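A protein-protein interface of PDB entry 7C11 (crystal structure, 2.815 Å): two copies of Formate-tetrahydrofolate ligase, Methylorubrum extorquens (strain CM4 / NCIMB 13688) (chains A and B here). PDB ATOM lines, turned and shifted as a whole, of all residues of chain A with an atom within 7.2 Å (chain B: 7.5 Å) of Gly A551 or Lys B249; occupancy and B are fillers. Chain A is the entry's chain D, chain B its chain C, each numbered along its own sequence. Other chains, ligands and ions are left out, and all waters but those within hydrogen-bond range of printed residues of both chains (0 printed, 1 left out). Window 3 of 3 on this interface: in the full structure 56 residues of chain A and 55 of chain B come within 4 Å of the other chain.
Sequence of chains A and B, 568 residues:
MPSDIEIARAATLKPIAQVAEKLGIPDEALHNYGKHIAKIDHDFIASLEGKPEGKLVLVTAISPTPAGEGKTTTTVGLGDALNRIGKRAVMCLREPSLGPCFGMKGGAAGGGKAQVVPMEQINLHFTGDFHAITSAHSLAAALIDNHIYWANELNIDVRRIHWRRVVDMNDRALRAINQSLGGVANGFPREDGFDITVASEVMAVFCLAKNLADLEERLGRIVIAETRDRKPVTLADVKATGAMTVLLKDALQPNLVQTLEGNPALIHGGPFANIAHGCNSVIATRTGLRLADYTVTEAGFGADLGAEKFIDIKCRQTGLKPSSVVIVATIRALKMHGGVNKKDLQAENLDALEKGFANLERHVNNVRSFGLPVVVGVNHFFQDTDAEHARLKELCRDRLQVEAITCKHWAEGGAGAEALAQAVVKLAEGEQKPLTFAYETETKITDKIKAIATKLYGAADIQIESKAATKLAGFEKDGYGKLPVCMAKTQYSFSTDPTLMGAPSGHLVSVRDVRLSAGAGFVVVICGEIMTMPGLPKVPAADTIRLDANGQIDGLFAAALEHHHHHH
Of the printed residues of chain B, His A125 touches Ala B132 and Leu B247. Printed residues of chain A within 4 Å of Ala B132: His A125. Printed residues of chain A within 4 Å of Leu B212: Leu A547. Printed residues of chain A within 4 Å of Val B246: Arg A546 (3.7 Å), Leu A547 (3.7 Å) and Ile A553 (3.8 Å). Printed residues of chain A within 4 Å of Lys B249: Gly A551 (3.1 Å). The nearest printed residue of chain B that does not touch Ile A553 is Lys B249 (4.8 Å).
No position is printed for both chains. Of the 8 pairs that touch across the chains among the printed residues, none has its exchanged pair printed and touching as well.
Among the printed residues, pairs that only touch across the chains: His A125 with Ala B132 (3.8 Å), Arg A546 with Val B246 (3.7 Å), Leu A547 with Leu B212 (3.6 Å), Leu A547 with Thr B245 (3.7 Å), Leu A547 with Val B246 (3.7 Å), Gly A551 with Lys B249 (3.1 Å) and Ile A553 with Val B246 (3.8 Å).
O of Leu B247 lies within hydrogen-bond range of NE2 of His A125 (2.8 Å).
A ring nitrogen (NE2) of His B42 is in hydrogen-bond range of the backbone carbonyl oxygen (O) of Lys B249, 3.0 Å away. The backbone carbonyl oxygen (O) of Arg A546 is in hydrogen-bond range of the backbone NH (N) of Asp A554 (3.0 Å). The backbone NH (N) of Gly A551 is in hydrogen-bond range of the side-chain carboxylate (OD1) of Asp A548 (3.5 Å).
Of the 20 printed residues of chain B, 6 touch a printed residue of chain A. Hydrophobic or aromatic side chains of chain B that line the printed part of chain A: Leu B212, Val B246 and Leu B247. Of the 11 printed residues of chain A, 5 touch a printed residue of chain B. Hydrophobic or aromatic side chains of chain A that line the printed part of chain B: His A125, Leu A547 and Ile A553.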
ATOM      1  N   GLU A 120       6.601   1.082 -17.008  1.00  0.00           N
ATOM      2  CA  GLU A 120       7.035   1.506 -18.361  1.00  0.00           C
ATOM      3  C   GLU A 120       6.029   1.035 -19.416  1.00  0.00           C
ATOM      4  O   GLU A 120       5.778   1.793 -20.363  1.00  0.00           O
ATOM      5  CB  GLU A 120       8.437   0.963 -18.664  1.00  0.00           C
ATOM      6  CG  GLU A 120       9.558   1.755 -18.024  1.00  0.00           C
ATOM      7  CD  GLU A 120      10.908   1.121 -18.250  1.00  0.00           C
ATOM      8  OE1 GLU A 120      10.987   0.132 -19.009  1.00  0.00           O
ATOM      9  OE2 GLU A 120      11.884   1.615 -17.686  1.00  0.00           O
ATOM     10  N   HIS A 125       2.927   1.362 -25.059  1.00  0.00           N
ATOM     11  CA  HIS A 125       2.064   0.313 -25.670  1.00  0.00           C
ATOM     12  C   HIS A 125       1.891  -0.788 -24.633  1.00  0.00           C
ATOM     13  O   HIS A 125       2.817  -1.623 -24.513  1.00  0.00           O
ATOM     14  CB  HIS A 125       2.679  -0.322 -26.927  1.00  0.00           C
ATOM     15  CG  HIS A 125       3.654   0.512 -27.667  1.00  0.00           C
ATOM     16  ND1 HIS A 125       3.256   1.455 -28.586  1.00  0.00           N
ATOM     17  CD2 HIS A 125       4.996   0.510 -27.667  1.00  0.00           C
ATOM     18  CE1 HIS A 125       4.314   2.017 -29.130  1.00  0.00           C
ATOM     19  NE2 HIS A 125       5.400   1.452 -28.571  1.00  0.00           N
ATOM     20  N   ARG A 546      15.461   9.031 -24.156  1.00  0.00           N
ATOM     21  CA  ARG A 546      16.591   8.294 -24.789  1.00  0.00           C
ATOM     22  C   ARG A 546      16.755   6.918 -24.127  1.00  0.00           C
ATOM     23  O   ARG A 546      16.162   6.673 -23.038  1.00  0.00           O
ATOM     24  CB  ARG A 546      17.897   9.101 -24.709  1.00  0.00           C
ATOM     25  CG  ARG A 546      18.177   9.728 -23.351  1.00  0.00           C
ATOM     26  CD  ARG A 546      19.591  10.271 -23.216  1.00  0.00           C
ATOM     27  NE  ARG A 546      19.671  11.492 -22.402  1.00  0.00           N
ATOM     28  CZ  ARG A 546      19.846  12.745 -22.868  1.00  0.00           C
ATOM     29  NH1 ARG A 546      19.962  12.985 -24.167  1.00  0.00           N
ATOM     30  NH2 ARG A 546      19.914  13.765 -22.026  1.00  0.00           N
ATOM     31  N   LEU A 547      17.478   6.032 -24.813  1.00  0.00           N
ATOM     32  CA  LEU A 547      18.093   4.827 -24.215  1.00  0.00           C
ATOM     33  C   LEU A 547      19.515   5.221 -23.801  1.00  0.00           C
ATOM     34  O   LEU A 547      20.216   5.801 -24.646  1.00  0.00           O
ATOM     35  CB  LEU A 547      18.122   3.669 -25.224  1.00  0.00           C
ATOM     36  CG  LEU A 547      16.789   3.220 -25.825  1.00  0.00           C
ATOM     37  CD1 LEU A 547      16.993   1.962 -26.657  1.00  0.00           C
ATOM     38  CD2 LEU A 547      15.733   2.983 -24.764  1.00  0.00           C
ATOM     39  N   ASP A 548      19.927   4.905 -22.564  1.00  0.00           N
ATOM     40  CA  ASP A 548      21.352   4.985 -22.136  1.00  0.00           C
ATOM     41  C   ASP A 548      22.124   3.753 -22.651  1.00  0.00           C
ATOM     42  O   ASP A 548      21.528   2.878 -23.368  1.00  0.00           O
ATOM     43  CB  ASP A 548      21.476   5.214 -20.623  1.00  0.00           C
ATOM     44  CG  ASP A 548      21.035   4.082 -19.700  1.00  0.00           C
ATOM     45  OD1 ASP A 548      21.314   2.903 -20.006  1.00  0.00           O
ATOM     46  OD2 ASP A 548      20.452   4.402 -18.643  1.00  0.00           O
ATOM     47  N   ALA A 549      23.418   3.692 -22.312  1.00  0.00           N
ATOM     48  CA  ALA A 549      24.350   2.573 -22.598  1.00  0.00           C
ATOM     49  C   ALA A 549      23.641   1.211 -22.483  1.00  0.00           C
ATOM     50  O   ALA A 549      23.546   0.513 -23.517  1.00  0.00           O
ATOM     51  CB  ALA A 549      25.530   2.658 -21.652  1.00  0.00           C
ATOM     52  N   ASN A 550      23.154   0.870 -21.281  1.00  0.00           N
ATOM     53  CA  ASN A 550      22.508  -0.430 -20.959  1.00  0.00           C
ATOM     54  C   ASN A 550      21.153  -0.574 -21.652  1.00  0.00           C
ATOM     55  O   ASN A 550      20.540  -1.607 -21.463  1.00  0.00           O
ATOM     56  CB  ASN A 550      22.272  -0.597 -19.456  1.00  0.00           C
ATOM     57  CG  ASN A 550      23.559  -0.545 -18.666  1.00  0.00           C
ATOM     58  OD1 ASN A 550      23.781   0.390 -17.896  1.00  0.00           O
ATOM     59  ND2 ASN A 550      24.426  -1.520 -18.883  1.00  0.00           N
ATOM     60  N   GLY A 551      20.673   0.443 -22.376  1.00  0.00           N
ATOM     61  CA  GLY A 551      19.337   0.449 -23.022  1.00  0.00           C
ATOM     62  C   GLY A 551      18.195   0.694 -22.036  1.00  0.00           C
ATOM     63  O   GLY A 551      17.069   0.302 -22.322  1.00  0.00           O
ATOM     64  N   GLN A 552      18.468   1.335 -20.906  1.00  0.00           N
ATOM     65  CA  GLN A 552      17.423   1.843 -19.986  1.00  0.00           C
ATOM     66  C   GLN A 552      16.731   3.026 -20.653  1.00  0.00           C
ATOM     67  O   GLN A 552      17.341   3.614 -21.548  1.00  0.00           O
ATOM     68  CB  GLN A 552      18.061   2.275 -18.670  1.00  0.00           C
ATOM     69  CG  GLN A 552      17.058   2.523 -17.562  1.00  0.00           C
ATOM     70  CD  GLN A 552      17.774   2.803 -16.267  1.00  0.00           C
ATOM     71  OE1 GLN A 552      17.635   2.066 -15.296  1.00  0.00           O
ATOM     72  NE2 GLN A 552      18.555   3.871 -16.260  1.00  0.00           N
ATOM     73  N   ILE A 553      15.529   3.378 -20.203  1.00  0.00           N
ATOM     74  CA  ILE A 553      14.779   4.579 -20.682  1.00  0.00           C
ATOM     75  C   ILE A 553      14.973   5.721 -19.673  1.00  0.00           C
ATOM     76  O   ILE A 553      14.569   5.544 -18.511  1.00  0.00           O
ATOM     77  CB  ILE A 553      13.287   4.218 -20.857  1.00  0.00           C
ATOM     78  CG1 ILE A 553      13.110   3.027 -21.800  1.00  0.00           C
ATOM     79  CG2 ILE A 553      12.456   5.429 -21.287  1.00  0.00           C
ATOM     80  CD1 ILE A 553      11.711   2.499 -21.831  1.00  0.00           C
ATOM     81  N   ASP A 554      15.566   6.842 -20.091  1.00  0.00           N
ATOM     82  CA  ASP A 554      15.659   8.077 -19.266  1.00  0.00           C
ATOM     83  C   ASP A 554      14.807   9.189 -19.879  1.00  0.00           C
ATOM     84  O   ASP A 554      14.779   9.292 -21.132  1.00  0.00           O
ATOM     85  CB  ASP A 554      17.085   8.622 -19.162  1.00  0.00           C
ATOM     86  CG  ASP A 554      18.086   7.617 -18.640  1.00  0.00           C
ATOM     87  OD1 ASP A 554      17.694   6.806 -17.746  1.00  0.00           O
ATOM     88  OD2 ASP A 554      19.242   7.637 -19.141  1.00  0.00           O
ATOM     89  N   LYS B  39       8.277 -12.760 -28.632  1.00  0.00           N
ATOM     90  CA  LYS B  39       9.412 -11.925 -29.105  1.00  0.00           C
ATOM     91  C   LYS B  39      10.708 -12.491 -28.498  1.00  0.00           C
ATOM     92  O   LYS B  39      10.661 -12.912 -27.304  1.00  0.00           O
ATOM     93  CB  LYS B  39       9.197 -10.461 -28.696  1.00  0.00           C
ATOM     94  CG  LYS B  39       8.451  -9.599 -29.701  1.00  0.00           C
ATOM     95  CD  LYS B  39       8.282  -8.177 -29.251  1.00  0.00           C
ATOM     96  CE  LYS B  39       7.488  -7.329 -30.216  1.00  0.00           C
ATOM     97  NZ  LYS B  39       8.221  -7.094 -31.481  1.00  0.00           N
ATOM     98  N   ASP B  41      14.294 -11.897 -26.856  1.00  0.00           N
ATOM     99  CA  ASP B  41      14.730 -10.791 -25.976  1.00  0.00           C
ATOM    100  C   ASP B  41      15.986 -10.154 -26.554  1.00  0.00           C
ATOM    101  O   ASP B  41      16.814 -10.870 -27.106  1.00  0.00           O
ATOM    102  CB  ASP B  41      14.953 -11.279 -24.549  1.00  0.00           C
ATOM    103  CG  ASP B  41      15.620 -10.231 -23.697  1.00  0.00           C
ATOM    104  OD1 ASP B  41      14.942  -9.258 -23.294  1.00  0.00           O
ATOM    105  OD2 ASP B  41      16.814 -10.383 -23.494  1.00  0.00           O
ATOM    106  N   HIS B  42      16.129  -8.849 -26.383  1.00  0.00           N
ATOM    107  CA  HIS B  42      17.267  -8.070 -26.933  1.00  0.00           C
ATOM    108  C   HIS B  42      18.606  -8.586 -26.369  1.00  0.00           C
ATOM    109  O   HIS B  42      19.575  -8.706 -27.155  1.00  0.00           O
ATOM    110  CB  HIS B  42      17.030  -6.583 -26.677  1.00  0.00           C
ATOM    111  CG  HIS B  42      16.327  -5.917 -27.802  1.00  0.00           C
ATOM    112  ND1 HIS B  42      16.739  -6.095 -29.122  1.00  0.00           N
ATOM    113  CD2 HIS B  42      15.276  -5.065 -27.824  1.00  0.00           C
ATOM    114  CE1 HIS B  42      15.943  -5.392 -29.915  1.00  0.00           C
ATOM    115  NE2 HIS B  42      15.038  -4.745 -29.142  1.00  0.00           N
ATOM    116  N   ASP B  43      18.665  -8.863 -25.060  1.00  0.00           N
ATOM    117  CA  ASP B  43      19.898  -9.293 -24.346  1.00  0.00           C
ATOM    118  C   ASP B  43      20.309 -10.690 -24.840  1.00  0.00           C
ATOM    119  O   ASP B  43      21.557 -10.992 -24.872  1.00  0.00           O
ATOM    120  CB  ASP B  43      19.710  -9.260 -22.823  1.00  0.00           C
ATOM    121  CG  ASP B  43      19.947  -7.897 -22.200  1.00  0.00           C
ATOM    122  OD1 ASP B  43      20.628  -7.043 -22.862  1.00  0.00           O
ATOM    123  OD2 ASP B  43      19.475  -7.705 -21.049  1.00  0.00           O
ATOM    124  N   ALA B 132       3.794   0.509 -33.371  1.00  0.00           N
ATOM    125  CA  ALA B 132       4.961   1.204 -32.785  1.00  0.00           C
ATOM    126  C   ALA B 132       5.567   2.197 -33.798  1.00  0.00           C
ATOM    127  O   ALA B 132       5.937   3.306 -33.417  1.00  0.00           O
ATOM    128  CB  ALA B 132       5.963   0.168 -32.346  1.00  0.00           C
ATOM    129  N   PHE B 206      13.828   0.444 -39.816  1.00  0.00           N
ATOM    130  CA  PHE B 206      13.623  -0.635 -38.813  1.00  0.00           C
ATOM    131  C   PHE B 206      14.121  -1.968 -39.391  1.00  0.00           C
ATOM    132  O   PHE B 206      14.792  -2.750 -38.650  1.00  0.00           O
ATOM    133  CB  PHE B 206      12.146  -0.639 -38.425  1.00  0.00           C
ATOM    134  CG  PHE B 206      11.635  -1.637 -37.422  1.00  0.00           C
ATOM    135  CD1 PHE B 206      11.058  -2.824 -37.835  1.00  0.00           C
ATOM    136  CD2 PHE B 206      11.565  -1.304 -36.077  1.00  0.00           C
ATOM    137  CE1 PHE B 206      10.507  -3.704 -36.915  1.00  0.00           C
ATOM    138  CE2 PHE B 206      10.991  -2.170 -35.158  1.00  0.00           C
ATOM    139  CZ  PHE B 206      10.461  -3.371 -35.580  1.00  0.00           C
ATOM    140  N   LEU B 212      19.598  -1.294 -31.555  1.00  0.00           N
ATOM    141  CA  LEU B 212      18.998   0.009 -31.184  1.00  0.00           C
ATOM    142  C   LEU B 212      19.971   1.146 -31.473  1.00  0.00           C
ATOM    143  O   LEU B 212      19.484   2.252 -31.701  1.00  0.00           O
ATOM    144  CB  LEU B 212      18.618  -0.018 -29.709  1.00  0.00           C
ATOM    145  CG  LEU B 212      17.585  -1.069 -29.350  1.00  0.00           C
ATOM    146  CD1 LEU B 212      17.645  -1.410 -27.883  1.00  0.00           C
ATOM    147  CD2 LEU B 212      16.201  -0.601 -29.734  1.00  0.00           C
ATOM    148  N   LEU B 215      19.598   1.905 -35.244  1.00  0.00           N
ATOM    149  CA  LEU B 215      18.246   2.511 -35.425  1.00  0.00           C
ATOM    150  C   LEU B 215      18.330   4.024 -35.213  1.00  0.00           C
ATOM    151  O   LEU B 215      17.903   4.746 -36.109  1.00  0.00           O
ATOM    152  CB  LEU B 215      17.262   1.906 -34.414  1.00  0.00           C
ATOM    153  CG  LEU B 215      15.790   2.271 -34.605  1.00  0.00           C
ATOM    154  CD1 LEU B 215      15.197   1.577 -35.804  1.00  0.00           C
ATOM    155  CD2 LEU B 215      14.993   1.897 -33.379  1.00  0.00           C
ATOM    156  N   ALA B 243      13.358   9.309 -28.711  1.00  0.00           N
ATOM    157  CA  ALA B 243      11.981   8.928 -28.341  1.00  0.00           C
ATOM    158  C   ALA B 243      11.363   8.006 -29.412  1.00  0.00           C
ATOM    159  O   ALA B 243      10.667   7.024 -29.032  1.00  0.00           O
ATOM    160  CB  ALA B 243      11.148  10.176 -28.100  1.00  0.00           C
ATOM    161  N   MET B 244      11.587   8.275 -30.704  1.00  0.00           N
ATOM    162  CA  MET B 244      11.260   7.304 -31.794  1.00  0.00           C
ATOM    163  C   MET B 244      11.833   5.928 -31.413  1.00  0.00           C
ATOM    164  O   MET B 244      11.086   4.948 -31.504  1.00  0.00           O
ATOM    165  CB  MET B 244      11.797   7.767 -33.151  1.00  0.00           C
ATOM    166  CG  MET B 244      10.992   8.922 -33.718  1.00  0.00           C
ATOM    167  SD  MET B 244      11.638   9.715 -35.231  1.00  0.00           S
ATOM    168  CE  MET B 244      11.524   8.382 -36.420  1.00  0.00           C
ATOM    169  N   THR B 245      13.087   5.875 -30.945  1.00  0.00           N
ATOM    170  CA  THR B 245      13.824   4.623 -30.638  1.00  0.00           C
ATOM    171  C   THR B 245      13.196   3.951 -29.416  1.00  0.00           C
ATOM    172  O   THR B 245      13.063   2.692 -29.369  1.00  0.00           O
ATOM    173  CB  THR B 245      15.308   4.899 -30.406  1.00  0.00           C
ATOM    174  OG1 THR B 245      15.910   5.092 -31.688  1.00  0.00           O
ATOM    175  CG2 THR B 245      16.018   3.765 -29.696  1.00  0.00           C
ATOM    176  N   VAL B 246      12.834   4.771 -28.443  1.00  0.00           N
ATOM    177  CA  VAL B 246      12.246   4.297 -27.164  1.00  0.00           C
ATOM    178  C   VAL B 246      10.918   3.584 -27.475  1.00  0.00           C
ATOM    179  O   VAL B 246      10.721   2.476 -26.948  1.00  0.00           O
ATOM    180  CB  VAL B 246      12.165   5.467 -26.165  1.00  0.00           C
ATOM    181  CG1 VAL B 246      11.346   5.142 -24.926  1.00  0.00           C
ATOM    182  CG2 VAL B 246      13.571   5.873 -25.767  1.00  0.00           C
ATOM    183  N   LEU B 247      10.103   4.154 -28.368  1.00  0.00           N
ATOM    184  CA  LEU B 247       8.779   3.630 -28.798  1.00  0.00           C
ATOM    185  C   LEU B 247       8.956   2.369 -29.642  1.00  0.00           C
ATOM    186  O   LEU B 247       7.987   1.589 -29.753  1.00  0.00           O
ATOM    187  CB  LEU B 247       8.077   4.718 -29.615  1.00  0.00           C
ATOM    188  CG  LEU B 247       7.408   5.820 -28.804  1.00  0.00           C
ATOM    189  CD1 LEU B 247       7.185   7.088 -29.641  1.00  0.00           C
ATOM    190  CD2 LEU B 247       6.112   5.294 -28.226  1.00  0.00           C
ATOM    191  N   LEU B 248      10.120   2.234 -30.276  1.00  0.00           N
ATOM    192  CA  LEU B 248      10.470   1.145 -31.222  1.00  0.00           C
ATOM    193  C   LEU B 248      11.293   0.044 -30.519  1.00  0.00           C
ATOM    194  O   LEU B 248      11.585  -0.961 -31.147  1.00  0.00           O
ATOM    195  CB  LEU B 248      11.249   1.789 -32.374  1.00  0.00           C
ATOM    196  CG  LEU B 248      10.435   2.572 -33.393  1.00  0.00           C
ATOM    197  CD1 LEU B 248      11.320   3.030 -34.525  1.00  0.00           C
ATOM    198  CD2 LEU B 248       9.299   1.748 -33.964  1.00  0.00           C
ATOM    199  N   LYS B 249      11.637   0.222 -29.244  1.00  0.00           N
ATOM    200  CA  LYS B 249      12.459  -0.734 -28.438  1.00  0.00           C
ATOM    201  C   LYS B 249      11.860  -2.154 -28.467  1.00  0.00           C
ATOM    202  O   LYS B 249      12.517  -3.052 -29.028  1.00  0.00           O
ATOM    203  CB  LYS B 249      12.616  -0.271 -26.985  1.00  0.00           C
ATOM    204  CG  LYS B 249      13.365  -1.260 -26.095  1.00  0.00           C
ATOM    205  CD  LYS B 249      13.789  -0.692 -24.740  1.00  0.00           C
ATOM    206  CE  LYS B 249      15.140  -1.205 -24.292  1.00  0.00           C
ATOM    207  NZ  LYS B 249      15.065  -2.589 -23.771  1.00  0.00           N
ATOM    208  N   ASP B 250      10.685  -2.376 -27.875  1.00  0.00           N
ATOM    209  CA  ASP B 250      10.066  -3.723 -27.838  1.00  0.00           C
ATOM    210  C   ASP B 250       9.955  -4.280 -29.258  1.00  0.00           C
ATOM    211  O   ASP B 250      10.263  -5.473 -29.446  1.00  0.00           O
ATOM    212  CB  ASP B 250       8.701  -3.674 -27.168  1.00  0.00           C
ATOM    213  CG  ASP B 250       8.802  -3.299 -25.699  1.00  0.00           C
ATOM    214  OD1 ASP B 250       9.948  -3.241 -25.195  1.00  0.00           O
ATOM    215  OD2 ASP B 250       7.746  -3.042 -25.081  1.00  0.00           O
ATOM    216  N   ALA B 251       9.559  -3.431 -30.217  1.00  0.00           N
ATOM    217  CA  ALA B 251       9.176  -3.804 -31.598  1.00  0.00           C
ATOM    218  C   ALA B 251      10.375  -4.374 -32.355  1.00  0.00           C
ATOM    219  O   ALA B 251      10.182  -5.314 -33.172  1.00  0.00           O
ATOM    220  CB  ALA B 251       8.580  -2.628 -32.317  1.00  0.00           C
ATOM    221  N   LEU B 252      11.576  -3.872 -32.099  1.00  0.00           N
ATOM    222  CA  LEU B 252      12.781  -4.288 -32.868  1.00  0.00           C
ATOM    223  C   LEU B 252      13.172  -5.731 -32.524  1.00  0.00           C
ATOM    224  O   LEU B 252      14.052  -6.273 -33.216  1.00  0.00           O
ATOM    225  CB  LEU B 252      13.932  -3.322 -32.571  1.00  0.00           C
ATOM    226  CG  LEU B 252      15.163  -3.515 -33.453  1.00  0.00           C
ATOM    227  CD1 LEU B 252      14.810  -3.311 -34.920  1.00  0.00           C
ATOM    228  CD2 LEU B 252      16.285  -2.588 -33.016  1.00  0.00           C
ATOM    229  N   GLN B 253      12.588  -6.324 -31.476  1.00  0.00           N
ATOM    230  CA  GLN B 253      12.739  -7.760 -31.157  1.00  0.00           C
ATOM    231  C   GLN B 253      11.923  -8.595 -32.142  1.00  0.00           C
ATOM    232  O   GLN B 253      10.706  -8.444 -32.218  1.00  0.00           O
ATOM    233  CB  GLN B 253      12.203  -8.032 -29.762  1.00  0.00           C
ATOM    234  CG  GLN B 253      12.989  -7.366 -28.655  1.00  0.00           C
ATOM    235  CD  GLN B 253      12.295  -7.498 -27.325  1.00  0.00           C
ATOM    236  OE1 GLN B 253      11.097  -7.252 -27.204  1.00  0.00           O
ATOM    237  NE2 GLN B 253      13.057  -7.878 -26.317  1.00  0.00           N
ATOM    238  N   HIS B 268       8.931 -10.258 -38.977  1.00  0.00           N
ATOM    239  CA  HIS B 268       9.433  -8.979 -38.456  1.00  0.00           C
ATOM    240  C   HIS B 268       9.711  -8.087 -39.648  1.00  0.00           C
ATOM    241  O   HIS B 268      10.514  -8.515 -40.480  1.00  0.00           O
ATOM    242  CB  HIS B 268      10.680  -9.216 -37.608  1.00  0.00           C
ATOM    243  CG  HIS B 268      10.963  -8.120 -36.640  1.00  0.00           C
ATOM    244  ND1 HIS B 268      12.238  -7.799 -36.243  1.00  0.00           N
ATOM    245  CD2 HIS B 268      10.136  -7.286 -35.981  1.00  0.00           C
ATOM    246  CE1 HIS B 268      12.184  -6.815 -35.374  1.00  0.00           C
ATOM    247  NE2 HIS B 268      10.906  -6.477 -35.198  1.00  0.00           N
